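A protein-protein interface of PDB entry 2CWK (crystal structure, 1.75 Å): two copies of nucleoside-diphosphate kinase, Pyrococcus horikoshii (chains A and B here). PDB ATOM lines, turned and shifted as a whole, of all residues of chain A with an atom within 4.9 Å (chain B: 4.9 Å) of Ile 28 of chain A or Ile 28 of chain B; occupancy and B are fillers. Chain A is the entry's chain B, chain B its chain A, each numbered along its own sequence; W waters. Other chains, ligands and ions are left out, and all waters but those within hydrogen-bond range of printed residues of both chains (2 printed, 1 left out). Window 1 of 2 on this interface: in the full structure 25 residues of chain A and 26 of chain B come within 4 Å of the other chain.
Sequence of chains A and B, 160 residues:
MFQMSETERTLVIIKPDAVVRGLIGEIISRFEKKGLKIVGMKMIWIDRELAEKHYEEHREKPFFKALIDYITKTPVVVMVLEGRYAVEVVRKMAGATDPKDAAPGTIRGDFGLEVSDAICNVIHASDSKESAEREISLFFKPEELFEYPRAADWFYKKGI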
ATOM      1  N   ILE A  14     -16.421 -24.486  17.509  1.00  0.00           N
ATOM      2  CA  ILE A  14     -17.388 -25.558  17.702  1.00  0.00           C
ATOM      3  C   ILE A  14     -18.623 -24.937  17.051  1.00  0.00           C
ATOM      4  O   ILE A  14     -19.238 -24.017  17.596  1.00  0.00           O
ATOM      5  CB  ILE A  14     -17.613 -25.844  19.200  1.00  0.00           C
ATOM      6  CG1 ILE A  14     -16.311 -26.366  19.815  1.00  0.00           C
ATOM      7  CG2 ILE A  14     -18.731 -26.862  19.376  1.00  0.00           C
ATOM      8  CD1 ILE A  14     -16.399 -26.691  21.302  1.00  0.00           C
ATOM      9  N   ILE A  24     -20.475 -29.782  22.895  1.00  0.00           N
ATOM     10  CA  ILE A  24     -19.380 -28.907  23.306  1.00  0.00           C
ATOM     11  C   ILE A  24     -18.384 -29.613  24.221  1.00  0.00           C
ATOM     12  O   ILE A  24     -17.187 -29.649  23.937  1.00  0.00           O
ATOM     13  CB  ILE A  24     -19.902 -27.647  24.040  1.00  0.00           C
ATOM     14  CG1 ILE A  24     -20.791 -26.826  23.101  1.00  0.00           C
ATOM     15  CG2 ILE A  24     -18.727 -26.804  24.529  1.00  0.00           C
ATOM     16  CD1 ILE A  24     -21.417 -25.609  23.758  1.00  0.00           C
ATOM     17  N   GLY A  25     -18.886 -30.177  25.314  1.00  0.00           N
ATOM     18  CA  GLY A  25     -18.021 -30.853  26.264  1.00  0.00           C
ATOM     19  C   GLY A  25     -17.246 -32.025  25.696  1.00  0.00           C
ATOM     20  O   GLY A  25     -16.056 -32.177  25.966  1.00  0.00           O
ATOM     21  N   GLU A  26     -17.928 -32.858  24.917  1.00  0.00           N
ATOM     22  CA  GLU A  26     -17.321 -34.036  24.304  1.00  0.00           C
ATOM     23  C   GLU A  26     -16.138 -33.638  23.421  1.00  0.00           C
ATOM     24  O   GLU A  26     -15.093 -34.286  23.423  1.00  0.00           O
ATOM     25  CB  GLU A  26     -18.364 -34.762  23.453  1.00  0.00           C
ATOM     26  CG  GLU A  26     -18.158 -36.258  23.324  1.00  0.00           C
ATOM     27  CD  GLU A  26     -18.660 -37.012  24.536  1.00  0.00           C
ATOM     28  OE1 GLU A  26     -18.089 -36.832  25.631  1.00  0.00           O
ATOM     29  OE2 GLU A  26     -19.634 -37.782  24.394  1.00  0.00           O
ATOM     30  N   ILE A  27     -16.318 -32.567  22.661  1.00  0.00           N
ATOM     31  CA  ILE A  27     -15.276 -32.077  21.770  1.00  0.00           C
ATOM     32  C   ILE A  27     -14.092 -31.520  22.555  1.00  0.00           C
ATOM     33  O   ILE A  27     -12.941 -31.864  22.290  1.00  0.00           O
ATOM     34  CB  ILE A  27     -15.844 -30.994  20.834  1.00  0.00           C
ATOM     35  CG1 ILE A  27     -16.878 -31.630  19.900  1.00  0.00           C
ATOM     36  CG2 ILE A  27     -14.712 -30.322  20.052  1.00  0.00           C
ATOM     37  CD1 ILE A  27     -17.662 -30.643  19.051  1.00  0.00           C
ATOM     38  N   ILE A  28     -14.377 -30.667  23.532  1.00  0.00           N
ATOM     39  CA  ILE A  28     -13.319 -30.082  24.343  1.00  0.00           C
ATOM     40  C   ILE A  28     -12.505 -31.164  25.052  1.00  0.00           C
ATOM     41  O   ILE A  28     -11.277 -31.081  25.113  1.00  0.00           O
ATOM     42  CB  ILE A  28     -13.901 -29.103  25.388  1.00  0.00           C
ATOM     43  CG1 ILE A  28     -14.453 -27.867  24.672  1.00  0.00           C
ATOM     44  CG2 ILE A  28     -12.832 -28.710  26.411  1.00  0.00           C
ATOM     45  CD1 ILE A  28     -15.105 -26.859  25.595  1.00  0.00           C
ATOM     46  N   SER A  29     -13.181 -32.186  25.568  1.00  0.00           N
ATOM     47  CA  SER A  29     -12.485 -33.267  26.265  1.00  0.00           C
ATOM     48  C   SER A  29     -11.474 -33.978  25.375  1.00  0.00           C
ATOM     49  O   SER A  29     -10.424 -34.420  25.847  1.00  0.00           O
ATOM     50  CB  SER A  29     -13.481 -34.291  26.814  1.00  0.00           C
ATOM     51  OG  SER A  29     -14.172 -33.783  27.939  1.00  0.00           O
ATOM     52  N   ARG A  30     -11.779 -34.097  24.089  1.00  0.00           N
ATOM     53  CA  ARG A  30     -10.851 -34.765  23.189  1.00  0.00           C
ATOM     54  C   ARG A  30      -9.555 -33.983  23.071  1.00  0.00           C
ATOM     55  O   ARG A  30      -8.476 -34.566  22.985  1.00  0.00           O
ATOM     56  CB  ARG A  30     -11.481 -34.961  21.812  1.00  0.00           C
ATOM     57  CG  ARG A  30     -12.675 -35.886  21.854  1.00  0.00           C
ATOM     58  CD  ARG A  30     -13.002 -36.441  20.492  1.00  0.00           C
ATOM     59  NE  ARG A  30     -14.044 -37.455  20.581  1.00  0.00           N
ATOM     60  CZ  ARG A  30     -14.309 -38.337  19.625  1.00  0.00           C
ATOM     61  NH1 ARG A  30     -13.604 -38.328  18.501  1.00  0.00           N
ATOM     62  NH2 ARG A  30     -15.278 -39.225  19.792  1.00  0.00           N
ATOM     63  N   PHE A  31      -9.655 -32.659  23.071  1.00  0.00           N
ATOM     64  CA  PHE A  31      -8.457 -31.834  22.979  1.00  0.00           C
ATOM     65  C   PHE A  31      -7.680 -31.882  24.288  1.00  0.00           C
ATOM     66  O   PHE A  31      -6.453 -31.980  24.284  1.00  0.00           O
ATOM     67  CB  PHE A  31      -8.826 -30.390  22.648  1.00  0.00           C
ATOM     68  CG  PHE A  31      -9.487 -30.230  21.314  1.00  0.00           C
ATOM     69  CD1 PHE A  31      -8.905 -30.767  20.170  1.00  0.00           C
ATOM     70  CD2 PHE A  31     -10.690 -29.542  21.197  1.00  0.00           C
ATOM     71  CE1 PHE A  31      -9.512 -30.624  18.925  1.00  0.00           C
ATOM     72  CE2 PHE A  31     -11.304 -29.394  19.955  1.00  0.00           C
ATOM     73  CZ  PHE A  31     -10.715 -29.935  18.820  1.00  0.00           C
ATOM     74  N   GLU A  32      -8.393 -31.821  25.407  1.00  0.00           N
ATOM     75  CA  GLU A  32      -7.741 -31.854  26.711  1.00  0.00           C
ATOM     76  C   GLU A  32      -7.002 -33.163  26.966  1.00  0.00           C
ATOM     77  O   GLU A  32      -5.882 -33.154  27.478  1.00  0.00           O
ATOM     78  CB  GLU A  32      -8.757 -31.625  27.831  1.00  0.00           C
ATOM     79  CG  GLU A  32      -9.243 -30.192  27.943  1.00  0.00           C
ATOM     80  CD  GLU A  32     -10.295 -30.031  29.020  1.00  0.00           C
ATOM     81  OE1 GLU A  32     -11.357 -30.674  28.904  1.00  0.00           O
ATOM     82  OE2 GLU A  32     -10.064 -29.263  29.980  1.00  0.00           O
ATOM     83  N   ILE A  38      -6.058 -25.132  26.349  1.00  0.00           N
ATOM     84  CA  ILE A  38      -7.000 -24.106  25.926  1.00  0.00           C
ATOM     85  C   ILE A  38      -6.458 -22.796  26.488  1.00  0.00           C
ATOM     86  O   ILE A  38      -6.415 -22.609  27.704  1.00  0.00           O
ATOM     87  CB  ILE A  38      -8.401 -24.371  26.503  1.00  0.00           C
ATOM     88  CG1 ILE A  38      -8.919 -25.715  25.982  1.00  0.00           C
ATOM     89  CG2 ILE A  38      -9.345 -23.227  26.131  1.00  0.00           C
ATOM     90  CD1 ILE A  38     -10.181 -26.205  26.678  1.00  0.00           C
ATOM     91  N   MET A  41     -11.029 -18.962  25.073  1.00  0.00           N
ATOM     92  CA  MET A  41     -12.304 -19.567  24.721  1.00  0.00           C
ATOM     93  C   MET A  41     -13.482 -18.698  25.132  1.00  0.00           C
ATOM     94  O   MET A  41     -13.441 -18.017  26.155  1.00  0.00           O
ATOM     95  CB  MET A  41     -12.430 -20.948  25.378  1.00  0.00           C
ATOM     96  CG  MET A  41     -13.750 -21.644  25.103  1.00  0.00           C
ATOM     97  SD  MET A  41     -13.746 -23.348  25.691  1.00  0.00           S
ATOM     98  CE  MET A  41     -13.732 -23.099  27.453  1.00  0.00           C
ATOM     99  N   MET A  79     -12.341 -21.167  20.284  1.00  0.00           N
ATOM    100  CA  MET A  79     -11.269 -21.415  21.233  1.00  0.00           C
ATOM    101  C   MET A  79      -9.923 -21.526  20.547  1.00  0.00           C
ATOM    102  O   MET A  79      -9.829 -21.855  19.358  1.00  0.00           O
ATOM    103  CB  MET A  79     -11.552 -22.686  22.046  1.00  0.00           C
ATOM    104  CG  MET A  79     -11.686 -23.958  21.233  1.00  0.00           C
ATOM    105  SD  MET A  79     -12.198 -25.358  22.274  1.00  0.00           S
ATOM    106  CE  MET A  79     -13.889 -24.950  22.558  1.00  0.00           C
ATOM    107  N   ILE B  14     -15.684 -23.041  36.415  1.00  0.00           N
ATOM    108  CA  ILE B  14     -14.850 -24.233  36.394  1.00  0.00           C
ATOM    109  C   ILE B  14     -13.545 -23.664  36.950  1.00  0.00           C
ATOM    110  O   ILE B  14     -12.838 -22.910  36.277  1.00  0.00           O
ATOM    111  CB  ILE B  14     -14.686 -24.771  34.959  1.00  0.00           C
ATOM    112  CG1 ILE B  14     -16.065 -25.152  34.403  1.00  0.00           C
ATOM    113  CG2 ILE B  14     -13.765 -25.980  34.956  1.00  0.00           C
ATOM    114  CD1 ILE B  14     -16.047 -25.696  32.986  1.00  0.00           C
ATOM    115  N   ILE B  24     -12.336 -29.518  31.925  1.00  0.00           N
ATOM    116  CA  ILE B  24     -13.342 -28.597  31.398  1.00  0.00           C
ATOM    117  C   ILE B  24     -14.402 -29.332  30.580  1.00  0.00           C
ATOM    118  O   ILE B  24     -15.602 -29.162  30.801  1.00  0.00           O
ATOM    119  CB  ILE B  24     -12.702 -27.502  30.502  1.00  0.00           C
ATOM    120  CG1 ILE B  24     -11.755 -26.631  31.328  1.00  0.00           C
ATOM    121  CG2 ILE B  24     -13.795 -26.628  29.880  1.00  0.00           C
ATOM    122  CD1 ILE B  24     -10.941 -25.651  30.494  1.00  0.00           C
ATOM    123  N   GLY B  25     -13.950 -30.152  29.638  1.00  0.00           N
ATOM    124  CA  GLY B  25     -14.870 -30.883  28.785  1.00  0.00           C
ATOM    125  C   GLY B  25     -15.807 -31.826  29.515  1.00  0.00           C
ATOM    126  O   GLY B  25     -17.011 -31.835  29.257  1.00  0.00           O
ATOM    127  N   GLU B  26     -15.262 -32.630  30.422  1.00  0.00           N
ATOM    128  CA  GLU B  26     -16.077 -33.579  31.172  1.00  0.00           C
ATOM    129  C   GLU B  26     -17.169 -32.889  31.980  1.00  0.00           C
ATOM    130  O   GLU B  26     -18.300 -33.368  32.052  1.00  0.00           O
ATOM    131  CB  GLU B  26     -15.199 -34.412  32.106  1.00  0.00           C
ATOM    132  CG  GLU B  26     -14.303 -35.395  31.385  1.00  0.00           C
ATOM    133  CD  GLU B  26     -14.290 -36.749  32.056  1.00  0.00           C
ATOM    134  OE1 GLU B  26     -15.372 -37.369  32.156  1.00  0.00           O
ATOM    135  OE2 GLU B  26     -13.205 -37.193  32.486  1.00  0.00           O
ATOM    136  N   ILE B  27     -16.825 -31.762  32.590  1.00  0.00           N
ATOM    137  CA  ILE B  27     -17.784 -31.013  33.389  1.00  0.00           C
ATOM    138  C   ILE B  27     -18.898 -30.461  32.498  1.00  0.00           C
ATOM    139  O   ILE B  27     -20.084 -30.619  32.796  1.00  0.00           O
ATOM    140  CB  ILE B  27     -17.079 -29.857  34.143  1.00  0.00           C
ATOM    141  CG1 ILE B  27     -16.113 -30.444  35.179  1.00  0.00           C
ATOM    142  CG2 ILE B  27     -18.110 -28.959  34.820  1.00  0.00           C
ATOM    143  CD1 ILE B  27     -15.166 -29.421  35.797  1.00  0.00           C
ATOM    144  N   ILE B  28     -18.521 -29.825  31.396  1.00  0.00           N
ATOM    145  CA  ILE B  28     -19.517 -29.268  30.486  1.00  0.00           C
ATOM    146  C   ILE B  28     -20.456 -30.352  29.953  1.00  0.00           C
ATOM    147  O   ILE B  28     -21.671 -30.143  29.849  1.00  0.00           O
ATOM    148  CB  ILE B  28     -18.828 -28.539  29.308  1.00  0.00           C
ATOM    149  CG1 ILE B  28     -18.148 -27.269  29.831  1.00  0.00           C
ATOM    150  CG2 ILE B  28     -19.842 -28.210  28.221  1.00  0.00           C
ATOM    151  CD1 ILE B  28     -17.320 -26.531  28.790  1.00  0.00           C
ATOM    152  N   SER B  29     -19.902 -31.515  29.629  1.00  0.00           N
ATOM    153  CA  SER B  29     -20.717 -32.611  29.111  1.00  0.00           C
ATOM    154  C   SER B  29     -21.795 -33.040  30.095  1.00  0.00           C
ATOM    155  O   SER B  29     -22.901 -33.395  29.698  1.00  0.00           O
ATOM    156  CB  SER B  29     -19.841 -33.811  28.752  1.00  0.00           C
ATOM    157  OG  SER B  29     -19.045 -33.521  27.619  1.00  0.00           O
ATOM    158  N   ARG B  30     -21.487 -33.011  31.383  1.00  0.00           N
ATOM    159  CA  ARG B  30     -22.485 -33.412  32.366  1.00  0.00           C
ATOM    160  C   ARG B  30     -23.677 -32.466  32.345  1.00  0.00           C
ATOM    161  O   ARG B  30     -24.820 -32.895  32.482  1.00  0.00           O
ATOM    162  CB  ARG B  30     -21.865 -33.466  33.756  1.00  0.00           C
ATOM    163  CG  ARG B  30     -20.755 -34.490  33.826  1.00  0.00           C
ATOM    164  CD  ARG B  30     -20.491 -34.927  35.237  1.00  0.00           C
ATOM    165  NE  ARG B  30     -19.561 -36.048  35.271  1.00  0.00           N
ATOM    166  CZ  ARG B  30     -19.381 -36.825  36.332  1.00  0.00           C
ATOM    167  NH1 ARG B  30     -20.074 -36.594  37.439  1.00  0.00           N
ATOM    168  NH2 ARG B  30     -18.509 -37.824  36.285  1.00  0.00           N
ATOM    169  N   PHE B  31     -23.413 -31.178  32.161  1.00  0.00           N
ATOM    170  CA  PHE B  31     -24.500 -30.209  32.114  1.00  0.00           C
ATOM    171  C   PHE B  31     -25.299 -30.359  30.826  1.00  0.00           C
ATOM    172  O   PHE B  31     -26.529 -30.286  30.841  1.00  0.00           O
ATOM    173  CB  PHE B  31     -23.948 -28.789  32.236  1.00  0.00           C
ATOM    174  CG  PHE B  31     -23.290 -28.516  33.556  1.00  0.00           C
ATOM    175  CD1 PHE B  31     -23.952 -28.805  34.746  1.00  0.00           C
ATOM    176  CD2 PHE B  31     -22.013 -27.970  33.613  1.00  0.00           C
ATOM    177  CE1 PHE B  31     -23.354 -28.555  35.976  1.00  0.00           C
ATOM    178  CE2 PHE B  31     -21.404 -27.717  34.844  1.00  0.00           C
ATOM    179  CZ  PHE B  31     -22.076 -28.010  36.024  1.00  0.00           C
ATOM    180  N   GLU B  32     -24.599 -30.586  29.720  1.00  0.00           N
ATOM    181  CA  GLU B  32     -25.254 -30.757  28.425  1.00  0.00           C
ATOM    182  C   GLU B  32     -26.140 -32.000  28.382  1.00  0.00           C
ATOM    183  O   GLU B  32     -27.265 -31.949  27.881  1.00  0.00           O
ATOM    184  CB  GLU B  32     -24.213 -30.848  27.307  1.00  0.00           C
ATOM    185  CG  GLU B  32     -23.547 -29.531  26.958  1.00  0.00           C
ATOM    186  CD  GLU B  32     -22.503 -29.684  25.868  1.00  0.00           C
ATOM    187  OE1 GLU B  32     -21.501 -30.389  26.108  1.00  0.00           O
ATOM    188  OE2 GLU B  32     -22.684 -29.104  24.773  1.00  0.00           O
ATOM    189  N   ILE B  38     -26.123 -23.926  27.719  1.00  0.00           N
ATOM    190  CA  ILE B  38     -25.055 -22.969  27.981  1.00  0.00           C
ATOM    191  C   ILE B  38     -25.436 -21.707  27.217  1.00  0.00           C
ATOM    192  O   ILE B  38     -25.461 -21.713  25.988  1.00  0.00           O
ATOM    193  CB  ILE B  38     -23.697 -23.480  27.458  1.00  0.00           C
ATOM    194  CG1 ILE B  38     -23.302 -24.753  28.208  1.00  0.00           C
ATOM    195  CG2 ILE B  38     -22.636 -22.396  27.626  1.00  0.00           C
ATOM    196  CD1 ILE B  38     -22.131 -25.495  27.585  1.00  0.00           C
ATOM    197  N   MET B  41     -20.420 -18.170  28.078  1.00  0.00           N
ATOM    198  CA  MET B  41     -19.225 -18.858  28.540  1.00  0.00           C
ATOM    199  C   MET B  41     -17.958 -18.204  28.024  1.00  0.00           C
ATOM    200  O   MET B  41     -17.915 -17.699  26.903  1.00  0.00           O
ATOM    201  CB  MET B  41     -19.251 -20.322  28.095  1.00  0.00           C
ATOM    202  CG  MET B  41     -18.028 -21.115  28.523  1.00  0.00           C
ATOM    203  SD  MET B  41     -18.195 -22.870  28.144  1.00  0.00           S
ATOM    204  CE  MET B  41     -17.909 -22.856  26.385  1.00  0.00           C
ATOM    205  N   MET B  79     -19.353 -19.721  33.149  1.00  0.00           N
ATOM    206  CA  MET B  79     -20.429 -20.002  32.219  1.00  0.00           C
ATOM    207  C   MET B  79     -21.783 -19.887  32.884  1.00  0.00           C
ATOM    208  O   MET B  79     -21.918 -20.048  34.099  1.00  0.00           O
ATOM    209  CB  MET B  79     -20.253 -21.390  31.591  1.00  0.00           C
ATOM    210  CG  MET B  79     -20.314 -22.557  32.551  1.00  0.00           C
ATOM    211  SD  MET B  79     -19.972 -24.127  31.695  1.00  0.00           S
ATOM    212  CE  MET B  79     -19.835 -25.238  33.086  1.00  0.00           C
HETATM  213  O   HOH W   1     -12.330 -32.967  29.964  1.00  0.00           O
HETATM  214  O   HOH W   2     -20.831 -32.831  25.397  1.00  0.00           O
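Ile 24 of chain A touches Ile 38 of chain B, and with the chains exchanged Ile 38 of chain A touches Ile 24 of chain B. Gly 25 of chain A touches its own counterpart, Gly 25 of chain B. Gly 25 of chain A touches Ile 28 of chain B, and with the chains exchanged Ile 28 of chain A touches Gly 25 of chain B. Gly 25 of chain A touches Glu 32 of chain B, and with the chains exchanged Glu 32 of chain A touches Gly 25 of chain B. 13 positions are printed for both chains.
Hydrophobic or aromatic side chains of chain B that line the printed part of chain A: Ile 24, Ile 28 and Ile 38. Of the 13 printed residues of chain A, 7 touch a printed residue of chain B. Among the printed residues, no Asp or Glu carboxylate lies within 4 Å of a Lys or Arg side-chain nitrogen of the other chain.
N of Glu 26 of chain B lies within hydrogen-bond range of OG of Ser 29 of chain A (2.9 Å). N of Ile 24 of chain A sits at hydrogen-bond distance from OE2 of Glu 32 of chain B (3.0 Å). OE1 of Glu 32 of chain B sits at hydrogen-bond distance from N of Gly 25 of chain A, 2.7 Å away. N of Ile 24 of chain B lies within hydrogen-bond range of OE2 of Glu 32 of chain A, 3.0 Å away. N of Glu 26 of chain A lies within hydrogen-bond range of OG of Ser 29 of chain B. O of Gly 25 of chain B sits close to O of Gly 25 of chain A (3.4 Å). N of Gly 25 of chain B sits at hydrogen-bond distance from OE1 of Glu 32 of chain A (2.7 Å).
Printed residues of chain B within 4 Å of Ser 29 of chain A: Gly 25 (3.0 Å) and Glu 26 (2.9 Å). Phe 31 of chain A touches none of the printed residues of chain B. Of the printed residues of chain B, Ile 38 of chain A touches Ile 24 (3.9 Å). Of chain A, only Gly 25 and Ile 28 come within 4 Å of Ile 28 of chain B. Printed residues of chain A within 4 Å of Glu 32 of chain B: Ile 24 and Gly 25. The nearest residue of chain B that does not touch Ile 28 of chain A is Ile 24 of chain B (4.2 Å). The nearest residue of chain A that does not touch Ile 28 of chain B is Ile 24 of chain A (4.1 Å). The nearest printed residue of chain B that does not touch Ile 24 of chain A is Ile 28 of chain B (4.1 Å).
Water W2 lies within hydrogen-bond range of the side-chain carboxylate (OE1) of Glu 32 of chain B, the side-chain hydroxyl (OG) of Ser 29 of chain B, the backbone NH (N) of Glu 26 of chain A and the backbone NH (N) of Gly 25 of chain A. Water W1 lies within hydrogen-bond range of the side-chain carboxylate (OE1) of Glu 32 of chain A, the side-chain hydroxyl (OG) of Ser 29 of chain A, the backbone NH (N) of Glu 26 of chain B and the backbone NH (N) of Gly 25 of chain B.
Among the printed residues, pairs that only touch across the chains: Ser 29 of chain A with Gly 25 of chain B (3.0 Å), Gly 25 of chain A with Ser 29 of chain B (3.0 Å), Gly 25 of chain A with Ile 28 of chain B (3.6 Å), Ile 28 of chain A with Gly 25 of chain B (3.7 Å), Ile 24 of chain A with Ile 38 of chain B (3.9 Å), Ile 28 of chain A with Ile 28 of chain B (3.9 Å) and Ile 38 of chain A with Ile 24 of chain B (3.9 Å).
The backbone carbonyl oxygen (O) of Gly 25 of chain A sits at hydrogen-bond distance from the side-chain hydroxyl (OG) of Ser 29 of chain A (3.2 Å). O of Gly 25 of chain B lies within hydrogen-bond range of OG of Ser 29 of chain B (3.1 Å).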
